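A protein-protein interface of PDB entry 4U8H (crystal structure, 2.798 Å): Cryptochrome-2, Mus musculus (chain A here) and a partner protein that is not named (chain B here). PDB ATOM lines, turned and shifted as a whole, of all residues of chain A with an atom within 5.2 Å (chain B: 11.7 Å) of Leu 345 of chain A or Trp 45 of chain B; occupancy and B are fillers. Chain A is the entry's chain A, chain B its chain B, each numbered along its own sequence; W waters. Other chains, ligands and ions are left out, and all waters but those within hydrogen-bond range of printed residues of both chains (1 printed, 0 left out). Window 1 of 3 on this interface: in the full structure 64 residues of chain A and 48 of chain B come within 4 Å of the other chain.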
ATOM      1  N   VAL A  65      10.379  14.987 -14.782  1.00  0.00           N
ATOM      2  CA  VAL A  65      11.466  14.380 -15.543  1.00  0.00           C
ATOM      3  C   VAL A  65      12.379  13.443 -14.687  1.00  0.00           C
ATOM      4  O   VAL A  65      13.268  12.752 -15.200  1.00  0.00           O
ATOM      5  CB  VAL A  65      12.190  15.537 -16.258  1.00  0.00           C
ATOM      6  CG1 VAL A  65      13.636  15.297 -16.458  1.00  0.00           C
ATOM      7  CG2 VAL A  65      11.476  15.883 -17.560  1.00  0.00           C
ATOM      8  N   ARG A 340      24.417  33.024 -20.706  1.00  0.00           N
ATOM      9  CA  ARG A 340      23.058  32.581 -20.455  1.00  0.00           C
ATOM     10  C   ARG A 340      22.402  32.317 -21.817  1.00  0.00           C
ATOM     11  O   ARG A 340      22.582  33.090 -22.751  1.00  0.00           O
ATOM     12  CB  ARG A 340      22.280  33.614 -19.640  1.00  0.00           C
ATOM     13  CG  ARG A 340      20.908  33.133 -19.151  1.00  0.00           C
ATOM     14  CD  ARG A 340      21.024  32.190 -17.946  1.00  0.00           C
ATOM     15  NE  ARG A 340      19.884  31.277 -17.831  1.00  0.00           N
ATOM     16  CZ  ARG A 340      19.915  29.981 -18.151  1.00  0.00           C
ATOM     17  NH1 ARG A 340      21.036  29.416 -18.605  1.00  0.00           N
ATOM     18  NH2 ARG A 340      18.822  29.242 -18.012  1.00  0.00           N
ATOM     19  N   ASN A 341      21.702  31.190 -21.941  1.00  0.00           N
ATOM     20  CA  ASN A 341      20.914  30.864 -23.131  1.00  0.00           C
ATOM     21  C   ASN A 341      19.949  29.723 -22.791  1.00  0.00           C
ATOM     22  O   ASN A 341      20.272  28.555 -22.960  1.00  0.00           O
ATOM     23  CB  ASN A 341      21.828  30.508 -24.309  1.00  0.00           C
ATOM     24  CG  ASN A 341      21.067  30.342 -25.623  1.00  0.00           C
ATOM     25  OD1 ASN A 341      19.906  29.929 -25.636  1.00  0.00           O
ATOM     26  ND2 ASN A 341      21.728  30.649 -26.735  1.00  0.00           N
ATOM     27  N   PRO A 342      18.756  30.064 -22.293  1.00  0.00           N
ATOM     28  CA  PRO A 342      17.891  29.040 -21.696  1.00  0.00           C
ATOM     29  C   PRO A 342      17.387  28.058 -22.733  1.00  0.00           C
ATOM     30  O   PRO A 342      17.042  26.922 -22.399  1.00  0.00           O
ATOM     31  CB  PRO A 342      16.727  29.858 -21.118  1.00  0.00           C
ATOM     32  CG  PRO A 342      17.249  31.272 -21.034  1.00  0.00           C
ATOM     33  CD  PRO A 342      18.165  31.405 -22.201  1.00  0.00           C
ATOM     34  N   GLU A 343      17.365  28.509 -23.984  1.00  0.00           N
ATOM     35  CA  GLU A 343      16.858  27.724 -25.099  1.00  0.00           C
ATOM     36  C   GLU A 343      17.923  26.703 -25.465  1.00  0.00           C
ATOM     37  O   GLU A 343      17.618  25.579 -25.870  1.00  0.00           O
ATOM     38  CB  GLU A 343      16.561  28.639 -26.299  1.00  0.00           C
ATOM     39  CG  GLU A 343      16.099  30.054 -25.915  1.00  0.00           C
ATOM     40  CD  GLU A 343      14.808  30.043 -25.108  1.00  0.00           C
ATOM     41  OE1 GLU A 343      13.978  29.135 -25.332  1.00  0.00           O
ATOM     42  OE2 GLU A 343      14.622  30.934 -24.249  1.00  0.00           O
ATOM     43  N   ALA A 344      19.179  27.108 -25.308  1.00  0.00           N
ATOM     44  CA  ALA A 344      20.293  26.223 -25.580  1.00  0.00           C
ATOM     45  C   ALA A 344      20.346  25.127 -24.525  1.00  0.00           C
ATOM     46  O   ALA A 344      20.425  23.941 -24.851  1.00  0.00           O
ATOM     47  CB  ALA A 344      21.589  27.002 -25.605  1.00  0.00           C
ATOM     48  N   LEU A 345      20.299  25.537 -23.260  1.00  0.00           N
ATOM     49  CA  LEU A 345      20.296  24.600 -22.149  1.00  0.00           C
ATOM     50  C   LEU A 345      19.124  23.625 -22.267  1.00  0.00           C
ATOM     51  O   LEU A 345      19.255  22.451 -21.936  1.00  0.00           O
ATOM     52  CB  LEU A 345      20.243  25.359 -20.821  1.00  0.00           C
ATOM     53  CG  LEU A 345      19.882  24.584 -19.552  1.00  0.00           C
ATOM     54  CD1 LEU A 345      20.869  23.436 -19.279  1.00  0.00           C
ATOM     55  CD2 LEU A 345      19.821  25.520 -18.372  1.00  0.00           C
ATOM     56  N   ALA A 346      17.986  24.109 -22.753  1.00  0.00           N
ATOM     57  CA  ALA A 346      16.815  23.247 -22.925  1.00  0.00           C
ATOM     58  C   ALA A 346      17.025  22.234 -24.036  1.00  0.00           C
ATOM     59  O   ALA A 346      16.762  21.053 -23.844  1.00  0.00           O
ATOM     60  CB  ALA A 346      15.534  24.055 -23.154  1.00  0.00           C
ATOM     61  N   LYS A 347      17.505  22.687 -25.190  1.00  0.00           N
ATOM     62  CA  LYS A 347      17.761  21.774 -26.305  1.00  0.00           C
ATOM     63  C   LYS A 347      18.757  20.676 -25.913  1.00  0.00           C
ATOM     64  O   LYS A 347      18.584  19.499 -26.263  1.00  0.00           O
ATOM     65  CB  LYS A 347      18.251  22.535 -27.546  1.00  0.00           C
ATOM     66  CG  LYS A 347      17.138  23.273 -28.319  1.00  0.00           C
ATOM     67  CD  LYS A 347      17.695  24.182 -29.419  1.00  0.00           C
ATOM     68  CE  LYS A 347      17.930  23.444 -30.734  1.00  0.00           C
ATOM     69  NZ  LYS A 347      16.741  23.419 -31.650  1.00  0.00           N
ATOM     70  N   TRP A 348      19.791  21.069 -25.174  1.00  0.00           N
ATOM     71  CA  TRP A 348      20.747  20.116 -24.612  1.00  0.00           C
ATOM     72  C   TRP A 348      20.005  19.138 -23.718  1.00  0.00           C
ATOM     73  O   TRP A 348      19.963  17.947 -23.999  1.00  0.00           O
ATOM     74  CB  TRP A 348      21.814  20.865 -23.822  1.00  0.00           C
ATOM     75  CG  TRP A 348      22.857  20.021 -23.153  1.00  0.00           C
ATOM     76  CD1 TRP A 348      23.978  19.508 -23.721  1.00  0.00           C
ATOM     77  CD2 TRP A 348      22.905  19.652 -21.766  1.00  0.00           C
ATOM     78  NE1 TRP A 348      24.707  18.815 -22.789  1.00  0.00           N
ATOM     79  CE2 TRP A 348      24.071  18.884 -21.580  1.00  0.00           C
ATOM     80  CE3 TRP A 348      22.062  19.876 -20.669  1.00  0.00           C
ATOM     81  CZ2 TRP A 348      24.418  18.329 -20.342  1.00  0.00           C
ATOM     82  CZ3 TRP A 348      22.411  19.332 -19.437  1.00  0.00           C
ATOM     83  CH2 TRP A 348      23.577  18.567 -19.284  1.00  0.00           C
ATOM     84  N   ALA A 349      19.386  19.664 -22.666  1.00  0.00           N
ATOM     85  CA  ALA A 349      18.718  18.852 -21.656  1.00  0.00           C
ATOM     86  C   ALA A 349      17.767  17.841 -22.263  1.00  0.00           C
ATOM     87  O   ALA A 349      17.697  16.700 -21.794  1.00  0.00           O
ATOM     88  CB  ALA A 349      17.989  19.734 -20.655  1.00  0.00           C
ATOM     89  N   GLU A 350      17.062  18.253 -23.319  1.00  0.00           N
ATOM     90  CA  GLU A 350      16.043  17.406 -23.954  1.00  0.00           C
ATOM     91  C   GLU A 350      16.594  16.403 -24.959  1.00  0.00           C
ATOM     92  O   GLU A 350      15.929  15.422 -25.299  1.00  0.00           O
ATOM     93  CB  GLU A 350      14.934  18.243 -24.602  1.00  0.00           C
ATOM     94  CG  GLU A 350      13.992  18.914 -23.601  1.00  0.00           C
ATOM     95  CD  GLU A 350      13.440  17.950 -22.550  1.00  0.00           C
ATOM     96  OE1 GLU A 350      14.137  17.706 -21.538  1.00  0.00           O
ATOM     97  OE2 GLU A 350      12.308  17.440 -22.722  1.00  0.00           O
ATOM     98  N   LEU A 383      28.253  21.294 -23.695  1.00  0.00           N
ATOM     99  CA  LEU A 383      27.452  22.312 -23.040  1.00  0.00           C
ATOM    100  C   LEU A 383      28.338  23.396 -22.460  1.00  0.00           C
ATOM    101  O   LEU A 383      28.006  24.579 -22.510  1.00  0.00           O
ATOM    102  CB  LEU A 383      26.623  21.679 -21.920  1.00  0.00           C
ATOM    103  CG  LEU A 383      25.689  22.577 -21.110  1.00  0.00           C
ATOM    104  CD1 LEU A 383      24.421  22.853 -21.894  1.00  0.00           C
ATOM    105  CD2 LEU A 383      25.387  21.965 -19.750  1.00  0.00           C
ATOM    106  N   VAL A 390      27.688  27.274 -21.672  1.00  0.00           N
ATOM    107  CA  VAL A 390      26.713  27.380 -20.562  1.00  0.00           C
ATOM    108  C   VAL A 390      27.338  26.881 -19.263  1.00  0.00           C
ATOM    109  O   VAL A 390      28.116  25.938 -19.290  1.00  0.00           O
ATOM    110  CB  VAL A 390      25.401  26.594 -20.842  1.00  0.00           C
ATOM    111  CG1 VAL A 390      24.526  26.518 -19.609  1.00  0.00           C
ATOM    112  CG2 VAL A 390      24.623  27.222 -21.995  1.00  0.00           C
ATOM    113  N   SER A 394      24.810  24.268 -14.222  1.00  0.00           N
ATOM    114  CA  SER A 394      23.527  23.954 -14.834  1.00  0.00           C
ATOM    115  C   SER A 394      23.480  22.496 -15.299  1.00  0.00           C
ATOM    116  O   SER A 394      22.449  21.830 -15.170  1.00  0.00           O
ATOM    117  CB  SER A 394      23.248  24.896 -16.009  1.00  0.00           C
ATOM    118  OG  SER A 394      22.571  26.068 -15.563  1.00  0.00           O
ATOM    119  N   ARG A 397      22.716  20.545 -12.369  1.00  0.00           N
ATOM    120  CA  ARG A 397      21.284  20.598 -12.105  1.00  0.00           C
ATOM    121  C   ARG A 397      20.535  19.569 -12.952  1.00  0.00           C
ATOM    122  O   ARG A 397      19.740  18.791 -12.428  1.00  0.00           O
ATOM    123  CB  ARG A 397      20.715  22.016 -12.331  1.00  0.00           C
ATOM    124  CG  ARG A 397      21.187  23.046 -11.309  1.00  0.00           C
ATOM    125  CD  ARG A 397      20.503  24.436 -11.444  1.00  0.00           C
ATOM    126  NE  ARG A 397      21.292  25.448 -10.736  1.00  0.00           N
ATOM    127  CZ  ARG A 397      22.035  26.386 -11.322  1.00  0.00           C
ATOM    128  NH1 ARG A 397      22.071  26.496 -12.647  1.00  0.00           N
ATOM    129  NH2 ARG A 397      22.736  27.234 -10.579  1.00  0.00           N
ATOM    130  N   VAL A 398      20.805  19.556 -14.255  1.00  0.00           N
ATOM    131  CA  VAL A 398      20.154  18.608 -15.154  1.00  0.00           C
ATOM    132  C   VAL A 398      20.415  17.156 -14.767  1.00  0.00           C
ATOM    133  O   VAL A 398      19.484  16.347 -14.785  1.00  0.00           O
ATOM    134  CB  VAL A 398      20.532  18.837 -16.626  1.00  0.00           C
ATOM    135  CG1 VAL A 398      20.032  17.696 -17.468  1.00  0.00           C
ATOM    136  CG2 VAL A 398      19.934  20.130 -17.132  1.00  0.00           C
ATOM    137  N   GLU A 401      18.672  15.569 -11.381  1.00  0.00           N
ATOM    138  CA  GLU A 401      17.369  14.916 -11.566  1.00  0.00           C
ATOM    139  C   GLU A 401      17.421  13.629 -12.432  1.00  0.00           C
ATOM    140  O   GLU A 401      16.594  12.722 -12.294  1.00  0.00           O
ATOM    141  CB  GLU A 401      16.348  15.901 -12.160  1.00  0.00           C
ATOM    142  CG  GLU A 401      15.495  16.654 -11.130  1.00  0.00           C
ATOM    143  CD  GLU A 401      14.363  15.823 -10.532  1.00  0.00           C
ATOM    144  OE1 GLU A 401      13.243  15.871 -11.080  1.00  0.00           O
ATOM    145  OE2 GLU A 401      14.583  15.139  -9.506  1.00  0.00           O
ATOM    146  N   GLN B  41       5.521  19.457 -12.416  1.00  0.00           N
ATOM    147  CA  GLN B  41       5.752  20.292 -13.584  1.00  0.00           C
ATOM    148  C   GLN B  41       7.128  20.034 -14.172  1.00  0.00           C
ATOM    149  O   GLN B  41       7.936  19.303 -13.604  1.00  0.00           O
ATOM    150  CB  GLN B  41       5.643  21.771 -13.205  1.00  0.00           C
ATOM    151  CG  GLN B  41       4.485  22.123 -12.300  1.00  0.00           C
ATOM    152  CD  GLN B  41       4.243  23.613 -12.249  1.00  0.00           C
ATOM    153  OE1 GLN B  41       5.077  24.375 -11.757  1.00  0.00           O
ATOM    154  NE2 GLN B  41       3.110  24.039 -12.767  1.00  0.00           N
ATOM    155  N   ASP B  42       7.398  20.673 -15.299  1.00  0.00           N
ATOM    156  CA  ASP B  42       8.699  20.592 -15.923  1.00  0.00           C
ATOM    157  C   ASP B  42       9.736  21.133 -14.996  1.00  0.00           C
ATOM    158  O   ASP B  42       9.439  21.965 -14.155  1.00  0.00           O
ATOM    159  CB  ASP B  42       8.719  21.412 -17.196  1.00  0.00           C
ATOM    160  CG  ASP B  42       8.071  20.710 -18.318  1.00  0.00           C
ATOM    161  OD1 ASP B  42       8.102  19.465 -18.298  1.00  0.00           O
ATOM    162  OD2 ASP B  42       7.521  21.395 -19.200  1.00  0.00           O
ATOM    163  N   PRO B  43      10.971  20.666 -15.152  1.00  0.00           N
ATOM    164  CA  PRO B  43      12.033  21.240 -14.325  1.00  0.00           C
ATOM    165  C   PRO B  43      12.298  22.688 -14.746  1.00  0.00           C
ATOM    166  O   PRO B  43      11.808  23.124 -15.789  1.00  0.00           O
ATOM    167  CB  PRO B  43      13.223  20.340 -14.624  1.00  0.00           C
ATOM    168  CG  PRO B  43      12.899  19.688 -15.978  1.00  0.00           C
ATOM    169  CD  PRO B  43      11.427  19.588 -16.052  1.00  0.00           C
ATOM    170  N   ILE B  44      13.065  23.410 -13.939  1.00  0.00           N
ATOM    171  CA  ILE B  44      13.304  24.832 -14.141  1.00  0.00           C
ATOM    172  C   ILE B  44      13.890  25.155 -15.509  1.00  0.00           C
ATOM    173  O   ILE B  44      13.526  26.156 -16.109  1.00  0.00           O
ATOM    174  CB  ILE B  44      14.235  25.381 -13.062  1.00  0.00           C
ATOM    175  CG1 ILE B  44      13.732  24.946 -11.693  1.00  0.00           C
ATOM    176  CG2 ILE B  44      14.306  26.867 -13.147  1.00  0.00           C
ATOM    177  CD1 ILE B  44      14.718  25.207 -10.607  1.00  0.00           C
ATOM    178  N   TRP B  45      14.795  24.314 -16.004  1.00  0.00           N
ATOM    179  CA  TRP B  45      15.457  24.589 -17.285  1.00  0.00           C
ATOM    180  C   TRP B  45      14.478  24.620 -18.467  1.00  0.00           C
ATOM    181  O   TRP B  45      14.732  25.264 -19.486  1.00  0.00           O
ATOM    182  CB  TRP B  45      16.647  23.638 -17.546  1.00  0.00           C
ATOM    183  CG  TRP B  45      16.373  22.153 -17.407  1.00  0.00           C
ATOM    184  CD1 TRP B  45      15.971  21.292 -18.385  1.00  0.00           C
ATOM    185  CD2 TRP B  45      16.524  21.365 -16.223  1.00  0.00           C
ATOM    186  NE1 TRP B  45      15.840  20.021 -17.875  1.00  0.00           N
ATOM    187  CE2 TRP B  45      16.180  20.041 -16.550  1.00  0.00           C
ATOM    188  CE3 TRP B  45      16.885  21.657 -14.911  1.00  0.00           C
ATOM    189  CZ2 TRP B  45      16.199  19.013 -15.614  1.00  0.00           C
ATOM    190  CZ3 TRP B  45      16.890  20.642 -13.986  1.00  0.00           C
ATOM    191  CH2 TRP B  45      16.552  19.332 -14.338  1.00  0.00           C
ATOM    192  N   LEU B  46      13.346  23.947 -18.328  1.00  0.00           N
ATOM    193  CA  LEU B  46      12.340  24.019 -19.376  1.00  0.00           C
ATOM    194  C   LEU B  46      11.446  25.213 -19.193  1.00  0.00           C
ATOM    195  O   LEU B  46      11.257  25.995 -20.119  1.00  0.00           O
ATOM    196  CB  LEU B  46      11.494  22.749 -19.443  1.00  0.00           C
ATOM    197  CG  LEU B  46      12.273  21.524 -19.861  1.00  0.00           C
ATOM    198  CD1 LEU B  46      11.315  20.401 -20.093  1.00  0.00           C
ATOM    199  CD2 LEU B  46      13.088  21.846 -21.093  1.00  0.00           C
ATOM    200  N   LEU B  47      10.868  25.328 -18.003  1.00  0.00           N
ATOM    201  CA  LEU B  47       9.999  26.458 -17.663  1.00  0.00           C
ATOM    202  C   LEU B  47      10.573  27.839 -18.034  1.00  0.00           C
ATOM    203  O   LEU B  47       9.834  28.719 -18.463  1.00  0.00           O
ATOM    204  CB  LEU B  47       9.644  26.405 -16.177  1.00  0.00           C
ATOM    205  CG  LEU B  47       8.869  25.157 -15.745  1.00  0.00           C
ATOM    206  CD1 LEU B  47       8.529  25.172 -14.263  1.00  0.00           C
ATOM    207  CD2 LEU B  47       7.605  24.990 -16.546  1.00  0.00           C
ATOM    208  N   MET B  48      11.885  28.013 -17.882  1.00  0.00           N
ATOM    209  CA  MET B  48      12.566  29.265 -18.224  1.00  0.00           C
ATOM    210  C   MET B  48      12.869  29.433 -19.719  1.00  0.00           C
ATOM    211  O   MET B  48      13.457  30.420 -20.137  1.00  0.00           O
ATOM    212  CB  MET B  48      13.877  29.394 -17.430  1.00  0.00           C
ATOM    213  CG  MET B  48      13.718  29.346 -15.923  1.00  0.00           C
ATOM    214  SD  MET B  48      12.214  30.177 -15.382  1.00  0.00           S
ATOM    215  CE  MET B  48      12.772  31.842 -15.153  1.00  0.00           C
ATOM    216  N   ALA B  49      12.461  28.471 -20.524  1.00  0.00           N
ATOM    217  CA  ALA B  49      12.872  28.436 -21.912  1.00  0.00           C
ATOM    218  C   ALA B  49      11.670  28.290 -22.819  1.00  0.00           C
ATOM    219  O   ALA B  49      10.702  27.618 -22.474  1.00  0.00           O
ATOM    220  CB  ALA B  49      13.822  27.270 -22.137  1.00  0.00           C
ATOM    221  N   ASN B  50      11.733  28.919 -23.983  1.00  0.00           N
ATOM    222  CA  ASN B  50      10.719  28.708 -24.997  1.00  0.00           C
ATOM    223  C   ASN B  50      11.020  27.393 -25.697  1.00  0.00           C
ATOM    224  O   ASN B  50      11.976  27.301 -26.459  1.00  0.00           O
ATOM    225  CB  ASN B  50      10.711  29.859 -25.999  1.00  0.00           C
ATOM    226  CG  ASN B  50       9.625  29.712 -27.034  1.00  0.00           C
ATOM    227  OD1 ASN B  50       8.558  29.157 -26.757  1.00  0.00           O
ATOM    228  ND2 ASN B  50       9.888  30.202 -28.239  1.00  0.00           N
ATOM    229  N   THR B  51      10.213  26.373 -25.417  1.00  0.00           N
ATOM    230  CA  THR B  51      10.468  25.038 -25.936  1.00  0.00           C
ATOM    231  C   THR B  51       9.364  24.575 -26.854  1.00  0.00           C
ATOM    232  O   THR B  51       8.898  23.444 -26.728  1.00  0.00           O
ATOM    233  CB  THR B  51      10.586  23.989 -24.817  1.00  0.00           C
ATOM    234  OG1 THR B  51       9.454  24.090 -23.958  1.00  0.00           O
ATOM    235  CG2 THR B  51      11.836  24.193 -23.991  1.00  0.00           C
ATOM    236  N   ASP B  52       8.926  25.433 -27.768  1.00  0.00           N
ATOM    237  CA  ASP B  52       7.985  24.981 -28.797  1.00  0.00           C
ATOM    238  C   ASP B  52       8.752  24.580 -30.055  1.00  0.00           C
ATOM    239  O   ASP B  52       9.898  25.003 -30.233  1.00  0.00           O
ATOM    240  CB  ASP B  52       6.881  26.014 -29.093  1.00  0.00           C
ATOM    241  CG  ASP B  52       7.427  27.396 -29.381  1.00  0.00           C
ATOM    242  OD1 ASP B  52       8.603  27.491 -29.788  1.00  0.00           O
ATOM    243  OD2 ASP B  52       6.677  28.387 -29.198  1.00  0.00           O
ATOM    244  N   ILE B  55      11.759  26.243 -31.779  1.00  0.00           N
ATOM    245  CA  ILE B  55      12.999  26.323 -31.001  1.00  0.00           C
ATOM    246  C   ILE B  55      13.659  24.938 -30.890  1.00  0.00           C
ATOM    247  O   ILE B  55      14.868  24.778 -31.059  1.00  0.00           O
ATOM    248  CB  ILE B  55      12.777  26.924 -29.594  1.00  0.00           C
ATOM    249  CG1 ILE B  55      12.224  28.352 -29.690  1.00  0.00           C
ATOM    250  CG2 ILE B  55      14.077  26.902 -28.800  1.00  0.00           C
ATOM    251  CD1 ILE B  55      13.279  29.416 -29.841  1.00  0.00           C
ATOM    252  N   MET B  56      12.843  23.932 -30.617  1.00  0.00           N
ATOM    253  CA  MET B  56      13.343  22.581 -30.514  1.00  0.00           C
ATOM    254  C   MET B  56      13.851  22.068 -31.863  1.00  0.00           C
ATOM    255  O   MET B  56      14.963  21.544 -31.970  1.00  0.00           O
ATOM    256  CB  MET B  56      12.253  21.667 -29.958  1.00  0.00           C
ATOM    257  CG  MET B  56      11.879  21.951 -28.507  1.00  0.00           C
ATOM    258  SD  MET B  56      13.242  21.768 -27.326  1.00  0.00           S
ATOM    259  CE  MET B  56      13.556  23.476 -26.908  1.00  0.00           C
ATOM    260  N   TYR B  59      15.914  26.021 -33.825  1.00  0.00           N
ATOM    261  CA  TYR B  59      16.610  27.200 -33.307  1.00  0.00           C
ATOM    262  C   TYR B  59      18.101  27.064 -33.551  1.00  0.00           C
ATOM    263  O   TYR B  59      18.668  25.984 -33.390  1.00  0.00           O
ATOM    264  CB  TYR B  59      16.333  27.434 -31.818  1.00  0.00           C
ATOM    265  CG  TYR B  59      17.250  28.457 -31.158  1.00  0.00           C
ATOM    266  CD1 TYR B  59      17.070  29.824 -31.357  1.00  0.00           C
ATOM    267  CD2 TYR B  59      18.286  28.055 -30.325  1.00  0.00           C
ATOM    268  CE1 TYR B  59      17.906  30.757 -30.747  1.00  0.00           C
ATOM    269  CE2 TYR B  59      19.118  28.974 -29.719  1.00  0.00           C
ATOM    270  CZ  TYR B  59      18.926  30.321 -29.930  1.00  0.00           C
ATOM    271  OH  TYR B  59      19.765  31.225 -29.321  1.00  0.00           O
ATOM    272  N   GLN B  60      18.724  28.170 -33.948  1.00  0.00           N
ATOM    273  CA  GLN B  60      20.157  28.213 -34.218  1.00  0.00           C
ATOM    274  C   GLN B  60      20.839  29.179 -33.259  1.00  0.00           C
ATOM    275  O   GLN B  60      20.226  30.136 -32.795  1.00  0.00           O
ATOM    276  CB  GLN B  60      20.407  28.686 -35.655  1.00  0.00           C
ATOM    277  CG  GLN B  60      19.573  27.981 -36.730  1.00  0.00           C
ATOM    278  CD  GLN B  60      20.322  26.850 -37.412  1.00  0.00           C
ATOM    279  OE1 GLN B  60      20.956  26.025 -36.753  1.00  0.00           O
ATOM    280  NE2 GLN B  60      20.253  26.809 -38.742  1.00  0.00           N
ATOM    281  N   LEU B  61      22.110  28.941 -32.960  1.00  0.00           N
ATOM    282  CA  LEU B  61      22.869  29.909 -32.182  1.00  0.00           C
ATOM    283  C   LEU B  61      23.332  31.007 -33.131  1.00  0.00           C
ATOM    284  O   LEU B  61      23.406  30.778 -34.339  1.00  0.00           O
ATOM    285  CB  LEU B  61      24.050  29.243 -31.478  1.00  0.00           C
ATOM    286  CG  LEU B  61      23.663  28.616 -30.138  1.00  0.00           C
ATOM    287  CD1 LEU B  61      22.714  27.457 -30.326  1.00  0.00           C
ATOM    288  CD2 LEU B  61      24.865  28.188 -29.339  1.00  0.00           C
ATOM    289  N   PRO B  62      23.628  32.205 -32.599  1.00  0.00           N
ATOM    290  CA  PRO B  62      24.048  33.317 -33.460  1.00  0.00           C
ATOM    291  C   PRO B  62      25.442  33.113 -34.046  1.00  0.00           C
ATOM    292  O   PRO B  62      26.202  32.266 -33.568  1.00  0.00           O
ATOM    293  CB  PRO B  62      24.079  34.496 -32.493  1.00  0.00           C
ATOM    294  CG  PRO B  62      24.416  33.867 -31.174  1.00  0.00           C
ATOM    295  CD  PRO B  62      23.621  32.595 -31.177  1.00  0.00           C
HETATM  296  O   HOH W   1      16.893  26.634 -19.665  1.00  0.00           O
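The side-chain hydroxyl of Tyr 59 of chain B sits at hydrogen-bond distance from the side-chain amide nitrogen of Asn 341 of chain A, 3.3 Å away. The backbone carbonyl oxygen of Met 56 of chain B sits at hydrogen-bond distance from the side-chain amino group of Lys 347 of chain A (2.6 Å). The backbone NH (N) of Tyr 59 of chain B lies close to the side-chain amino group (NZ) of Lys 347 of chain A, at 3.5 Å. The side-chain amino group (NZ) of Lys 347 of chain A sits close to the backbone carbonyl oxygen (O) of Ile 55 of chain B, at 2.4 Å. The backbone NH (N) of Asn 50 of chain B lies within hydrogen-bond range of the side-chain carboxylate (OE1) of Glu 343 of chain A (2.6 Å).
The side-chain amide oxygen (OD1) of Asn 50 of chain B lies close to the side-chain carboxylate (OD2) of Asp 52 of chain B, 3.2 Å away. NH1 of Arg 397 of chain A lies within hydrogen-bond range of OG of Ser 394 of chain A. The side-chain amide oxygen (OD1) of Asn 341 of chain A lies close to the backbone NH (N) of Glu 343 of chain A (3.3 Å). N of Ala 344 of chain A lies within hydrogen-bond range of OD1 of Asn 341 of chain A.
Among the printed residues, merely in contact across the chains: Pro 342 of chain A with Ala 49 of chain B (3.2 Å), Ala 349 of chain A with Trp 45 of chain B (3.4 Å), Pro 342 of chain A with Met 48 of chain B (3.5 Å), Glu 343 of chain A with Ala 49 of chain B (3.5 Å), Arg 397 of chain A with Trp 45 of chain B (3.7 Å), Val 398 of chain A with Trp 45 of chain B (3.7 Å), Leu 345 of chain A with Trp 45 of chain B (3.8 Å), Ala 346 of chain A with Ala 49 of chain B (3.8 Å), Ala 346 of chain A with Thr 51 of chain B (3.8 Å), Ala 346 of chain A with Leu 46 of chain B (3.9 Å), Glu 343 of chain A with Ile 55 of chain B (3.9 Å), Ala 346 of chain A with Trp 45 of chain B (3.9 Å) and Glu 350 of chain A with Leu 46 of chain B (3.96 Å).
Of chain B, only Tyr 59 (3.3 Å) comes within 4 Å of Asn 341 of chain A. Leu 345 of chain A touches just one residue of chain B: Trp 45. Of chain B, only Trp 45 (3.9 Å), Leu 46 (3.9 Å), Ala 49 (3.8 Å) and Thr 51 (3.8 Å) come within 4 Å of Ala 346 of chain A. Of the printed residues of chain B, Glu 350 of chain A touches Leu 46 (3.96 Å). Printed residues of chain A within 4 Å of Trp 45 of chain B: Leu 345 (3.8 Å), Ala 346 (3.9 Å), Ala 349 (3.4 Å), Arg 397 (3.7 Å) and Val 398 (3.7 Å). Of the printed residues of chain A, Met 48 of chain B touches Pro 342 (3.5 Å). Printed residues of chain A within 4 Å of Met 56 of chain B: Lys 347. The nearest residue of chain B that does not touch Leu 345 of chain A is Leu 46 of chain B (6.3 Å). The nearest printed residue of chain A that does not touch Trp 45 of chain B is Glu 401 of chain A (4.1 Å).
Printed residues of chain B that touch a printed residue of chain A: Trp 45, Leu 46, Met 48, Ala 49, Asn 50, Thr 51, Ile 55, Met 56 and Tyr 59. Of the 18 printed residues of chain A, 10 touch a printed residue of chain B. Among the printed residues, no Asp or Glu carboxylate lies within 4 Å of a Lys or Arg side-chain nitrogen of the other chain.
Water W1 lies within hydrogen-bond range of the backbone carbonyl oxygen (O) of Trp 45 of chain B and the backbone carbonyl oxygen (O) of Pro 342 of chain A.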
